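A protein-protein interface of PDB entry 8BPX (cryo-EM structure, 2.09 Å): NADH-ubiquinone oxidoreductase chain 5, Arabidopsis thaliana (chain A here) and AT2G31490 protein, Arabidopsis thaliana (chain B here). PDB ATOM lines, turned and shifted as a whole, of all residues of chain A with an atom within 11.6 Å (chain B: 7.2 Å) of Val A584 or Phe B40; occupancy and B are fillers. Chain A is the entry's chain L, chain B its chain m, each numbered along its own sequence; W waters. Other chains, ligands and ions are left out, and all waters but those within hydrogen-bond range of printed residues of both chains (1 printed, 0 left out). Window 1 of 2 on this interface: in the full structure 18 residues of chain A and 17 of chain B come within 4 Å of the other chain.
Arg A575 touches none of the printed residues of chain B. Of the printed residues of chain B, Arg A579 touches Arg B32. Printed residues of chain B within 4 Å of Phe A580: Phe B40. Of the printed residues of chain B, Glu A583 touches Arg B32. Of the printed residues of chain B, Val A584 touches Leu B36 and Phe B40. Glu A587 touches none of the printed residues of chain B. Of the printed residues of chain B, Ala A593 touches Ile B37. Printed residues of chain A within 4 Å of Arg B32: Arg A579 (3.8 Å) and Glu A583 (2.8 Å). Gly B38 touches none of the printed residues of chain A. Phe B40 touches two residues of chain A. No residue of chain A comes within 4 Å of Gly B41. No residue of chain A comes within 4 Å of Ala B43. No residue of chain A comes within 4 Å of Leu B44. The nearest printed residue of chain B that does not touch Val A584 is Arg B32 (5.9 Å). The nearest printed residue of chain B that does not touch Ala A593 is Gly B41 (7.7 Å).
Water W1 lies within hydrogen-bond range of O of Glu A583 (2.6 Å), OE1 of Glu A587 (3.3 Å) and NH1 of Arg B32 (3.4 Å).
NH2 of Arg A579 touches NH2 of Arg B32, at 3.8 Å. Phe B40 touches Phe A580. CG2 of Val A584 touches CD2 of Leu B36 (3.99 Å). Val A584 touches Phe B40 (CG1 to CB, 3.6 Å). CD1 of Ile B37 touches O of Ala A588 (3.6 Å). Ala A593 touches Ile B37.
The guanidinium group of Arg B32 lies within salt-bridge range of the side-chain carboxylate of Glu A583 (2.8 Å).
Of the 22 printed residues of chain A, 6 touch a printed residue of chain B. Printed residues of chain A that touch a printed residue of chain B: Arg A579, Phe A580, Glu A583, Val A584, Ala A588 and Ala A593. Hydrophobic or aromatic side chains of chain A within 4 Å of the printed part of chain B: Phe A580, Val A584 and Ala A593. Of the 13 printed residues of chain B, 4 touch a printed residue of chain A. Hydrophobic or aromatic side chains of chain B within 4 Å of the printed part of chain A: Leu B36, Ile B37 and Phe B40. Among the printed residues, 7 pairs touch across the chains. Among the printed residues, Asp or Glu carboxylates within 4 Å of a Lys or Arg side-chain nitrogen of the other chain: Glu A583 with Arg B32.
The backbone carbonyl oxygen (O) of Ala A588 lies within hydrogen-bond range of the backbone NH (N) of Ala A593 (2.9 Å). The backbone NH of Leu A589 is in hydrogen-bond range of the backbone carbonyl oxygen of Val A584 (2.9 Å). The backbone carbonyl oxygen of Glu A583 sits at hydrogen-bond distance from the backbone NH of Ala A588. NH2 of Arg A579 lies within salt-bridge range of OE1 of Glu A583 (2.7 Å). The backbone carbonyl oxygen (O) of Phe A580 sits at hydrogen-bond distance from the backbone NH (N) of Ser A585. The backbone NH (N) of Ile B42 sits at hydrogen-bond distance from the backbone carbonyl oxygen (O) of Ile B37, at 3.4 Å.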
ATOM      1  N   PHE A 572     -26.970 -29.413 -12.106  1.00  0.00           N
ATOM      2  CA  PHE A 572     -25.625 -29.659 -12.595  1.00  0.00           C
ATOM      3  C   PHE A 572     -24.887 -28.413 -13.065  1.00  0.00           C
ATOM      4  O   PHE A 572     -23.660 -28.455 -13.168  1.00  0.00           O
ATOM      5  CB  PHE A 572     -25.654 -30.687 -13.735  1.00  0.00           C
ATOM      6  CG  PHE A 572     -25.999 -32.079 -13.287  1.00  0.00           C
ATOM      7  CD1 PHE A 572     -27.322 -32.482 -13.188  1.00  0.00           C
ATOM      8  CD2 PHE A 572     -25.004 -32.990 -12.967  1.00  0.00           C
ATOM      9  CE1 PHE A 572     -27.644 -33.762 -12.783  1.00  0.00           C
ATOM     10  CE2 PHE A 572     -25.320 -34.271 -12.560  1.00  0.00           C
ATOM     11  CZ  PHE A 572     -26.645 -34.658 -12.466  1.00  0.00           C
ATOM     12  N   ARG A 575     -26.096 -24.772  -9.752  1.00  0.00           N
ATOM     13  CA  ARG A 575     -25.489 -25.133  -8.479  1.00  0.00           C
ATOM     14  C   ARG A 575     -23.974 -25.236  -8.599  1.00  0.00           C
ATOM     15  O   ARG A 575     -23.252 -24.849  -7.680  1.00  0.00           O
ATOM     16  CB  ARG A 575     -26.094 -26.438  -7.953  1.00  0.00           C
ATOM     17  CG  ARG A 575     -25.393 -26.979  -6.715  1.00  0.00           C
ATOM     18  CD  ARG A 575     -26.312 -27.606  -5.660  1.00  0.00           C
ATOM     19  NE  ARG A 575     -27.669 -27.911  -6.096  1.00  0.00           N
ATOM     20  CZ  ARG A 575     -28.002 -28.927  -6.882  1.00  0.00           C
ATOM     21  NH1 ARG A 575     -27.090 -29.750  -7.373  1.00  0.00           N
ATOM     22  NH2 ARG A 575     -29.284 -29.129  -7.169  1.00  0.00           N
ATOM     23  N   SER A 576     -23.474 -25.737  -9.731  1.00  0.00           N
ATOM     24  CA  SER A 576     -22.031 -25.821  -9.927  1.00  0.00           C
ATOM     25  C   SER A 576     -21.383 -24.443  -9.863  1.00  0.00           C
ATOM     26  O   SER A 576     -20.414 -24.235  -9.125  1.00  0.00           O
ATOM     27  CB  SER A 576     -21.716 -26.500 -11.260  1.00  0.00           C
ATOM     28  OG  SER A 576     -21.565 -27.893 -11.100  1.00  0.00           O
ATOM     29  N   PHE A 577     -21.908 -23.485 -10.633  1.00  0.00           N
ATOM     30  CA  PHE A 577     -21.350 -22.132 -10.594  1.00  0.00           C
ATOM     31  C   PHE A 577     -21.512 -21.483  -9.221  1.00  0.00           C
ATOM     32  O   PHE A 577     -20.576 -20.846  -8.715  1.00  0.00           O
ATOM     33  CB  PHE A 577     -21.962 -21.262 -11.692  1.00  0.00           C
ATOM     34  CG  PHE A 577     -21.431 -21.561 -13.061  1.00  0.00           C
ATOM     35  CD1 PHE A 577     -22.000 -22.526 -13.864  1.00  0.00           C
ATOM     36  CD2 PHE A 577     -20.346 -20.857 -13.549  1.00  0.00           C
ATOM     37  CE1 PHE A 577     -21.484 -22.790 -15.118  1.00  0.00           C
ATOM     38  CE2 PHE A 577     -19.838 -21.116 -14.800  1.00  0.00           C
ATOM     39  CZ  PHE A 577     -20.413 -22.085 -15.586  1.00  0.00           C
ATOM     40  N   LEU A 578     -22.681 -21.640  -8.598  1.00  0.00           N
ATOM     41  CA  LEU A 578     -22.901 -21.044  -7.286  1.00  0.00           C
ATOM     42  C   LEU A 578     -21.926 -21.603  -6.256  1.00  0.00           C
ATOM     43  O   LEU A 578     -21.380 -20.856  -5.437  1.00  0.00           O
ATOM     44  CB  LEU A 578     -24.342 -21.282  -6.849  1.00  0.00           C
ATOM     45  CG  LEU A 578     -25.373 -20.290  -7.383  1.00  0.00           C
ATOM     46  CD1 LEU A 578     -26.752 -20.649  -6.858  1.00  0.00           C
ATOM     47  CD2 LEU A 578     -25.000 -18.867  -6.999  1.00  0.00           C
ATOM     48  N   ARG A 579     -21.653 -22.898  -6.304  1.00  0.00           N
ATOM     49  CA  ARG A 579     -20.722 -23.551  -5.353  1.00  0.00           C
ATOM     50  C   ARG A 579     -19.280 -23.119  -5.603  1.00  0.00           C
ATOM     51  O   ARG A 579     -18.616 -22.898  -4.592  1.00  0.00           O
ATOM     52  CB  ARG A 579     -20.875 -25.074  -5.305  1.00  0.00           C
ATOM     53  CG  ARG A 579     -22.170 -25.525  -4.652  1.00  0.00           C
ATOM     54  CD  ARG A 579     -22.126 -27.026  -4.666  1.00  0.00           C
ATOM     55  NE  ARG A 579     -20.972 -27.419  -3.888  1.00  0.00           N
ATOM     56  CZ  ARG A 579     -20.460 -28.634  -3.878  1.00  0.00           C
ATOM     57  NH1 ARG A 579     -20.984 -29.574  -4.638  1.00  0.00           N
ATOM     58  NH2 ARG A 579     -19.413 -28.896  -3.128  1.00  0.00           N
ATOM     59  N   PHE A 580     -18.878 -22.957  -6.852  1.00  0.00           N
ATOM     60  CA  PHE A 580     -17.550 -22.449  -7.218  1.00  0.00           C
ATOM     61  C   PHE A 580     -17.362 -21.068  -6.624  1.00  0.00           C
ATOM     62  O   PHE A 580     -16.287 -20.838  -6.104  1.00  0.00           O
ATOM     63  CB  PHE A 580     -17.323 -22.377  -8.731  1.00  0.00           C
ATOM     64  CG  PHE A 580     -15.955 -22.011  -9.230  1.00  0.00           C
ATOM     65  CD1 PHE A 580     -15.581 -20.686  -9.366  1.00  0.00           C
ATOM     66  CD2 PHE A 580     -15.069 -22.994  -9.639  1.00  0.00           C
ATOM     67  CE1 PHE A 580     -14.331 -20.358  -9.859  1.00  0.00           C
ATOM     68  CE2 PHE A 580     -13.818 -22.661 -10.127  1.00  0.00           C
ATOM     69  CZ  PHE A 580     -13.453 -21.343 -10.242  1.00  0.00           C
ATOM     70  N   GLY A 581     -18.396 -20.256  -6.771  1.00  0.00           N
ATOM     71  CA  GLY A 581     -18.219 -18.895  -6.303  1.00  0.00           C
ATOM     72  C   GLY A 581     -17.802 -18.796  -4.849  1.00  0.00           C
ATOM     73  O   GLY A 581     -17.048 -17.896  -4.478  1.00  0.00           O
ATOM     74  N   TYR A 582     -18.275 -19.706  -3.977  1.00  0.00           N
ATOM     75  CA  TYR A 582     -17.954 -19.713  -2.514  1.00  0.00           C
ATOM     76  C   TYR A 582     -16.769 -20.641  -2.176  1.00  0.00           C
ATOM     77  O   TYR A 582     -15.785 -20.135  -1.727  1.00  0.00           O
ATOM     78  CB  TYR A 582     -19.196 -20.039  -1.653  1.00  0.00           C
ATOM     79  CG  TYR A 582     -18.926 -19.996  -0.172  1.00  0.00           C
ATOM     80  CD1 TYR A 582     -18.963 -18.794   0.510  1.00  0.00           C
ATOM     81  CD2 TYR A 582     -18.565 -21.131   0.534  1.00  0.00           C
ATOM     82  CE1 TYR A 582     -18.686 -18.724   1.859  1.00  0.00           C
ATOM     83  CE2 TYR A 582     -18.280 -21.079   1.888  1.00  0.00           C
ATOM     84  CZ  TYR A 582     -18.351 -19.869   2.552  1.00  0.00           C
ATOM     85  OH  TYR A 582     -18.082 -19.770   3.878  1.00  0.00           O
ATOM     86  N   GLU A 583     -16.845 -21.910  -2.509  1.00  0.00           N
ATOM     87  CA  GLU A 583     -15.824 -22.955  -2.217  1.00  0.00           C
ATOM     88  C   GLU A 583     -14.479 -22.875  -2.970  1.00  0.00           C
ATOM     89  O   GLU A 583     -13.536 -23.332  -2.408  1.00  0.00           O
ATOM     90  CB  GLU A 583     -16.489 -24.305  -2.394  1.00  0.00           C
ATOM     91  CG  GLU A 583     -17.621 -24.530  -1.415  1.00  0.00           C
ATOM     92  CD  GLU A 583     -18.672 -25.483  -1.936  1.00  0.00           C
ATOM     93  OE1 GLU A 583     -18.315 -26.630  -2.221  1.00  0.00           O
ATOM     94  OE2 GLU A 583     -19.838 -25.068  -2.074  1.00  0.00           O
ATOM     95  N   VAL A 584     -14.362 -22.219  -4.121  1.00  0.00           N
ATOM     96  CA  VAL A 584     -13.086 -22.234  -4.865  1.00  0.00           C
ATOM     97  C   VAL A 584     -12.507 -20.830  -4.930  1.00  0.00           C
ATOM     98  O   VAL A 584     -11.460 -20.619  -4.354  1.00  0.00           O
ATOM     99  CB  VAL A 584     -13.240 -22.922  -6.263  1.00  0.00           C
ATOM    100  CG1 VAL A 584     -11.972 -22.877  -7.088  1.00  0.00           C
ATOM    101  CG2 VAL A 584     -13.837 -24.310  -6.179  1.00  0.00           C
ATOM    102  N   SER A 585     -13.163 -19.958  -5.642  1.00  0.00           N
ATOM    103  CA  SER A 585     -12.762 -18.577  -5.886  1.00  0.00           C
ATOM    104  C   SER A 585     -12.581 -17.773  -4.587  1.00  0.00           C
ATOM    105  O   SER A 585     -11.619 -17.091  -4.510  1.00  0.00           O
ATOM    106  CB  SER A 585     -13.753 -17.955  -6.886  1.00  0.00           C
ATOM    107  OG  SER A 585     -15.045 -17.808  -6.362  1.00  0.00           O
ATOM    108  N   PHE A 586     -13.468 -17.982  -3.636  1.00  0.00           N
ATOM    109  CA  PHE A 586     -13.460 -17.200  -2.389  1.00  0.00           C
ATOM    110  C   PHE A 586     -12.714 -17.948  -1.268  1.00  0.00           C
ATOM    111  O   PHE A 586     -11.718 -17.423  -0.839  1.00  0.00           O
ATOM    112  CB  PHE A 586     -14.865 -16.745  -2.015  1.00  0.00           C
ATOM    113  CG  PHE A 586     -14.912 -15.839  -0.820  1.00  0.00           C
ATOM    114  CD1 PHE A 586     -14.341 -14.576  -0.870  1.00  0.00           C
ATOM    115  CD2 PHE A 586     -15.527 -16.248   0.348  1.00  0.00           C
ATOM    116  CE1 PHE A 586     -14.399 -13.735   0.227  1.00  0.00           C
ATOM    117  CE2 PHE A 586     -15.561 -15.409   1.449  1.00  0.00           C
ATOM    118  CZ  PHE A 586     -15.006 -14.158   1.383  1.00  0.00           C
ATOM    119  N   GLU A 587     -13.139 -19.127  -0.923  1.00  0.00           N
ATOM    120  CA  GLU A 587     -12.603 -19.924   0.210  1.00  0.00           C
ATOM    121  C   GLU A 587     -11.298 -20.673  -0.093  1.00  0.00           C
ATOM    122  O   GLU A 587     -10.412 -20.550   0.689  1.00  0.00           O
ATOM    123  CB  GLU A 587     -13.711 -20.810   0.748  1.00  0.00           C
ATOM    124  CG  GLU A 587     -13.310 -21.575   1.981  1.00  0.00           C
ATOM    125  CD  GLU A 587     -14.464 -22.341   2.586  1.00  0.00           C
ATOM    126  OE1 GLU A 587     -15.151 -23.053   1.848  1.00  0.00           O
ATOM    127  OE2 GLU A 587     -14.671 -22.204   3.788  1.00  0.00           O
ATOM    128  N   ALA A 588     -11.179 -21.412  -1.194  1.00  0.00           N
ATOM    129  CA  ALA A 588      -9.875 -22.067  -1.464  1.00  0.00           C
ATOM    130  C   ALA A 588      -8.816 -21.056  -1.929  1.00  0.00           C
ATOM    131  O   ALA A 588      -7.653 -21.246  -1.601  1.00  0.00           O
ATOM    132  CB  ALA A 588     -10.025 -23.188  -2.453  1.00  0.00           C
ATOM    133  N   LEU A 589      -9.211 -20.027  -2.672  1.00  0.00           N
ATOM    134  CA  LEU A 589      -8.217 -19.097  -3.285  1.00  0.00           C
ATOM    135  C   LEU A 589      -8.139 -17.785  -2.487  1.00  0.00           C
ATOM    136  O   LEU A 589      -7.267 -17.694  -1.621  1.00  0.00           O
ATOM    137  CB  LEU A 589      -8.576 -18.864  -4.754  1.00  0.00           C
ATOM    138  CG  LEU A 589      -8.353 -20.084  -5.648  1.00  0.00           C
ATOM    139  CD1 LEU A 589      -8.726 -19.805  -7.095  1.00  0.00           C
ATOM    140  CD2 LEU A 589      -6.921 -20.581  -5.543  1.00  0.00           C
ATOM    141  N   ASP A 590      -9.001 -16.820  -2.799  1.00  0.00           N
ATOM    142  CA  ASP A 590      -8.980 -15.444  -2.225  1.00  0.00           C
ATOM    143  C   ASP A 590      -8.768 -15.454  -0.712  1.00  0.00           C
ATOM    144  O   ASP A 590      -7.805 -14.822  -0.249  1.00  0.00           O
ATOM    145  CB  ASP A 590     -10.244 -14.679  -2.609  1.00  0.00           C
ATOM    146  CG  ASP A 590     -10.155 -14.033  -3.973  1.00  0.00           C
ATOM    147  OD1 ASP A 590     -10.951 -13.120  -4.239  1.00  0.00           O
ATOM    148  OD2 ASP A 590      -9.292 -14.455  -4.752  1.00  0.00           O
ATOM    149  N   LYS A 591      -9.646 -16.136   0.004  1.00  0.00           N
ATOM    150  CA  LYS A 591      -9.516 -16.205   1.452  1.00  0.00           C
ATOM    151  C   LYS A 591      -8.740 -17.427   1.921  1.00  0.00           C
ATOM    152  O   LYS A 591      -8.637 -17.652   3.130  1.00  0.00           O
ATOM    153  CB  LYS A 591     -10.899 -16.192   2.107  1.00  0.00           C
ATOM    154  CG  LYS A 591     -11.585 -14.840   2.072  1.00  0.00           C
ATOM    155  CD  LYS A 591     -10.970 -13.883   3.081  1.00  0.00           C
ATOM    156  CE  LYS A 591     -11.801 -12.625   3.225  1.00  0.00           C
ATOM    157  NZ  LYS A 591     -11.070 -11.558   3.963  1.00  0.00           N
ATOM    158  N   GLY A 592      -8.198 -18.217   1.003  1.00  0.00           N
ATOM    159  CA  GLY A 592      -7.458 -19.407   1.368  1.00  0.00           C
ATOM    160  C   GLY A 592      -5.977 -19.323   1.068  1.00  0.00           C
ATOM    161  O   GLY A 592      -5.212 -18.725   1.832  1.00  0.00           O
ATOM    162  N   ALA A 593      -5.548 -19.961  -0.022  1.00  0.00           N
ATOM    163  CA  ALA A 593      -4.131 -19.965  -0.474  1.00  0.00           C
ATOM    164  C   ALA A 593      -3.536 -18.557  -0.642  1.00  0.00           C
ATOM    165  O   ALA A 593      -2.384 -18.372  -0.229  1.00  0.00           O
ATOM    166  CB  ALA A 593      -3.961 -20.749  -1.754  1.00  0.00           C
ATOM    167  N   ILE A 594      -4.267 -17.618  -1.230  1.00  0.00           N
ATOM    168  CA  ILE A 594      -3.724 -16.260  -1.508  1.00  0.00           C
ATOM    169  C   ILE A 594      -3.572 -15.506  -0.179  1.00  0.00           C
ATOM    170  O   ILE A 594      -2.670 -14.682  -0.095  1.00  0.00           O
ATOM    171  CB  ILE A 594      -4.601 -15.506  -2.534  1.00  0.00           C
ATOM    172  CG1 ILE A 594      -4.724 -16.286  -3.846  1.00  0.00           C
ATOM    173  CG2 ILE A 594      -4.108 -14.090  -2.773  1.00  0.00           C
ATOM    174  CD1 ILE A 594      -5.807 -15.782  -4.765  1.00  0.00           C
ATOM    175  N   GLU A 595      -4.408 -15.801   0.821  1.00  0.00           N
ATOM    176  CA  GLU A 595      -4.221 -15.173   2.124  1.00  0.00           C
ATOM    177  C   GLU A 595      -3.026 -15.783   2.849  1.00  0.00           C
ATOM    178  O   GLU A 595      -2.210 -15.061   3.432  1.00  0.00           O
ATOM    179  CB  GLU A 595      -5.491 -15.324   2.963  1.00  0.00           C
ATOM    180  CG  GLU A 595      -6.269 -14.037   3.234  1.00  0.00           C
ATOM    181  CD  GLU A 595      -5.398 -12.828   3.496  1.00  0.00           C
ATOM    182  OE1 GLU A 595      -4.795 -12.736   4.582  1.00  0.00           O
ATOM    183  OE2 GLU A 595      -5.331 -11.951   2.612  1.00  0.00           O
ATOM    184  N   ARG B  32      -8.831 -31.942  -0.044  1.00  0.00           N
ATOM    185  CA  ARG B  32      -9.807 -31.249  -0.927  1.00  0.00           C
ATOM    186  C   ARG B  32      -9.228 -29.890  -1.330  1.00  0.00           C
ATOM    187  O   ARG B  32      -9.277 -29.565  -2.530  1.00  0.00           O
ATOM    188  CB  ARG B  32     -11.154 -31.075  -0.218  1.00  0.00           C
ATOM    189  CG  ARG B  32     -12.226 -30.425  -1.080  1.00  0.00           C
ATOM    190  CD  ARG B  32     -13.559 -30.305  -0.367  1.00  0.00           C
ATOM    191  NE  ARG B  32     -14.587 -29.749  -1.237  1.00  0.00           N
ATOM    192  CZ  ARG B  32     -14.921 -28.464  -1.293  1.00  0.00           C
ATOM    193  NH1 ARG B  32     -14.314 -27.582  -0.516  1.00  0.00           N
ATOM    194  NH2 ARG B  32     -15.867 -28.066  -2.124  1.00  0.00           N
ATOM    195  N   PHE B  34      -6.064 -28.962  -1.414  1.00  0.00           N
ATOM    196  CA  PHE B  34      -4.929 -29.181  -2.347  1.00  0.00           C
ATOM    197  C   PHE B  34      -5.484 -29.418  -3.754  1.00  0.00           C
ATOM    198  O   PHE B  34      -5.040 -28.736  -4.673  1.00  0.00           O
ATOM    199  CB  PHE B  34      -4.032 -30.335  -1.891  1.00  0.00           C
ATOM    200  CG  PHE B  34      -2.848 -29.906  -1.067  1.00  0.00           C
ATOM    201  CD1 PHE B  34      -2.702 -30.328   0.243  1.00  0.00           C
ATOM    202  CD2 PHE B  34      -1.892 -29.055  -1.592  1.00  0.00           C
ATOM    203  CE1 PHE B  34      -1.622 -29.916   1.006  1.00  0.00           C
ATOM    204  CE2 PHE B  34      -0.811 -28.644  -0.829  1.00  0.00           C
ATOM    205  CZ  PHE B  34      -0.677 -29.076   0.468  1.00  0.00           C
ATOM    206  N   ALA B  35      -6.472 -30.307  -3.883  1.00  0.00           N
ATOM    207  CA  ALA B  35      -7.011 -30.574  -5.212  1.00  0.00           C
ATOM    208  C   ALA B  35      -7.606 -29.314  -5.830  1.00  0.00           C
ATOM    209  O   ALA B  35      -7.350 -29.005  -6.998  1.00  0.00           O
ATOM    210  CB  ALA B  35      -8.055 -31.689  -5.145  1.00  0.00           C
ATOM    211  N   LEU B  36      -8.347 -28.540  -5.023  1.00  0.00           N
ATOM    212  CA  LEU B  36      -9.046 -27.358  -5.584  1.00  0.00           C
ATOM    213  C   LEU B  36      -8.029 -26.282  -6.004  1.00  0.00           C
ATOM    214  O   LEU B  36      -8.208 -25.701  -7.043  1.00  0.00           O
ATOM    215  CB  LEU B  36     -10.166 -26.848  -4.661  1.00  0.00           C
ATOM    216  CG  LEU B  36     -11.436 -27.678  -4.531  1.00  0.00           C
ATOM    217  CD1 LEU B  36     -12.385 -27.005  -3.557  1.00  0.00           C
ATOM    218  CD2 LEU B  36     -12.103 -27.887  -5.871  1.00  0.00           C
ATOM    219  N   ILE B  37      -6.934 -26.164  -5.275  1.00  0.00           N
ATOM    220  CA  ILE B  37      -5.933 -25.126  -5.624  1.00  0.00           C
ATOM    221  C   ILE B  37      -5.097 -25.654  -6.791  1.00  0.00           C
ATOM    222  O   ILE B  37      -4.751 -24.857  -7.655  1.00  0.00           O
ATOM    223  CB  ILE B  37      -5.100 -24.735  -4.387  1.00  0.00           C
ATOM    224  CG1 ILE B  37      -5.966 -24.015  -3.352  1.00  0.00           C
ATOM    225  CG2 ILE B  37      -3.880 -23.915  -4.764  1.00  0.00           C
ATOM    226  CD1 ILE B  37      -5.428 -24.097  -1.952  1.00  0.00           C
ATOM    227  N   GLY B  38      -4.823 -26.958  -6.827  1.00  0.00           N
ATOM    228  CA  GLY B  38      -4.102 -27.502  -7.962  1.00  0.00           C
ATOM    229  C   GLY B  38      -4.875 -27.412  -9.261  1.00  0.00           C
ATOM    230  O   GLY B  38      -4.293 -27.146 -10.315  1.00  0.00           O
ATOM    231  N   ILE B  39      -6.189 -27.621  -9.208  1.00  0.00           N
ATOM    232  CA  ILE B  39      -6.990 -27.632 -10.424  1.00  0.00           C
ATOM    233  C   ILE B  39      -7.277 -26.213 -10.897  1.00  0.00           C
ATOM    234  O   ILE B  39      -7.011 -25.862 -12.050  1.00  0.00           O
ATOM    235  CB  ILE B  39      -8.289 -28.424 -10.198  1.00  0.00           C
ATOM    236  CG1 ILE B  39      -7.986 -29.918 -10.067  1.00  0.00           C
ATOM    237  CG2 ILE B  39      -9.279 -28.167 -11.333  1.00  0.00           C
ATOM    238  CD1 ILE B  39      -8.982 -30.669  -9.227  1.00  0.00           C
ATOM    239  N   PHE B  40      -7.750 -25.376  -9.981  1.00  0.00           N
ATOM    240  CA  PHE B  40      -8.267 -24.038 -10.347  1.00  0.00           C
ATOM    241  C   PHE B  40      -7.231 -22.939 -10.194  1.00  0.00           C
ATOM    242  O   PHE B  40      -7.337 -21.958 -10.808  1.00  0.00           O
ATOM    243  CB  PHE B  40      -9.572 -23.813  -9.601  1.00  0.00           C
ATOM    244  CG  PHE B  40     -10.663 -24.748 -10.050  1.00  0.00           C
ATOM    245  CD1 PHE B  40     -11.174 -24.658 -11.336  1.00  0.00           C
ATOM    246  CD2 PHE B  40     -11.170 -25.719  -9.204  1.00  0.00           C
ATOM    247  CE1 PHE B  40     -12.178 -25.514 -11.761  1.00  0.00           C
ATOM    248  CE2 PHE B  40     -12.171 -26.575  -9.630  1.00  0.00           C
ATOM    249  CZ  PHE B  40     -12.677 -26.469 -10.906  1.00  0.00           C
ATOM    250  N   GLY B  41      -6.151 -23.177  -9.453  1.00  0.00           N
ATOM    251  CA  GLY B  41      -5.126 -22.136  -9.237  1.00  0.00           C
ATOM    252  C   GLY B  41      -3.885 -22.276 -10.096  1.00  0.00           C
ATOM    253  O   GLY B  41      -3.228 -21.260 -10.301  1.00  0.00           O
ATOM    254  N   ILE B  42      -3.571 -23.492 -10.563  1.00  0.00           N
ATOM    255  CA  ILE B  42      -2.430 -23.784 -11.481  1.00  0.00           C
ATOM    256  C   ILE B  42      -3.009 -24.283 -12.811  1.00  0.00           C
ATOM    257  O   ILE B  42      -2.817 -23.581 -13.809  1.00  0.00           O
ATOM    258  CB  ILE B  42      -1.417 -24.771 -10.839  1.00  0.00           C
ATOM    259  CG1 ILE B  42      -0.607 -24.092  -9.730  1.00  0.00           C
ATOM    260  CG2 ILE B  42      -0.513 -25.413 -11.872  1.00  0.00           C
ATOM    261  CD1 ILE B  42      -1.121 -24.356  -8.341  1.00  0.00           C
ATOM    262  N   ALA B  43      -3.710 -25.422 -12.811  1.00  0.00           N
ATOM    263  CA  ALA B  43      -3.952 -26.132 -14.064  1.00  0.00           C
ATOM    264  C   ALA B  43      -4.809 -25.314 -15.026  1.00  0.00           C
ATOM    265  O   ALA B  43      -4.433 -25.111 -16.185  1.00  0.00           O
ATOM    266  CB  ALA B  43      -4.600 -27.489 -13.786  1.00  0.00           C
ATOM    267  N   LEU B  44      -5.963 -24.831 -14.561  1.00  0.00           N
ATOM    268  CA  LEU B  44      -6.865 -24.092 -15.445  1.00  0.00           C
ATOM    269  C   LEU B  44      -6.232 -22.830 -16.024  1.00  0.00           C
ATOM    270  O   LEU B  44      -6.376 -22.600 -17.236  1.00  0.00           O
ATOM    271  CB  LEU B  44      -8.173 -23.778 -14.710  1.00  0.00           C
ATOM    272  CG  LEU B  44      -9.321 -23.248 -15.571  1.00  0.00           C
ATOM    273  CD1 LEU B  44      -9.402 -23.993 -16.900  1.00  0.00           C
ATOM    274  CD2 LEU B  44     -10.646 -23.316 -14.832  1.00  0.00           C
ATOM    275  N   PRO B  45      -5.551 -21.976 -15.248  1.00  0.00           N
ATOM    276  CA  PRO B  45      -4.836 -20.853 -15.880  1.00  0.00           C
ATOM    277  C   PRO B  45      -3.815 -21.289 -16.916  1.00  0.00           C
ATOM    278  O   PRO B  45      -3.678 -20.629 -17.950  1.00  0.00           O
ATOM    279  CB  PRO B  45      -4.174 -20.153 -14.687  1.00  0.00           C
ATOM    280  CG  PRO B  45      -5.027 -20.502 -13.537  1.00  0.00           C
ATOM    281  CD  PRO B  45      -5.483 -21.895 -13.778  1.00  0.00           C
HETATM  282  O   HOH W   1     -12.912 -24.470  -0.140  1.00  0.00           O
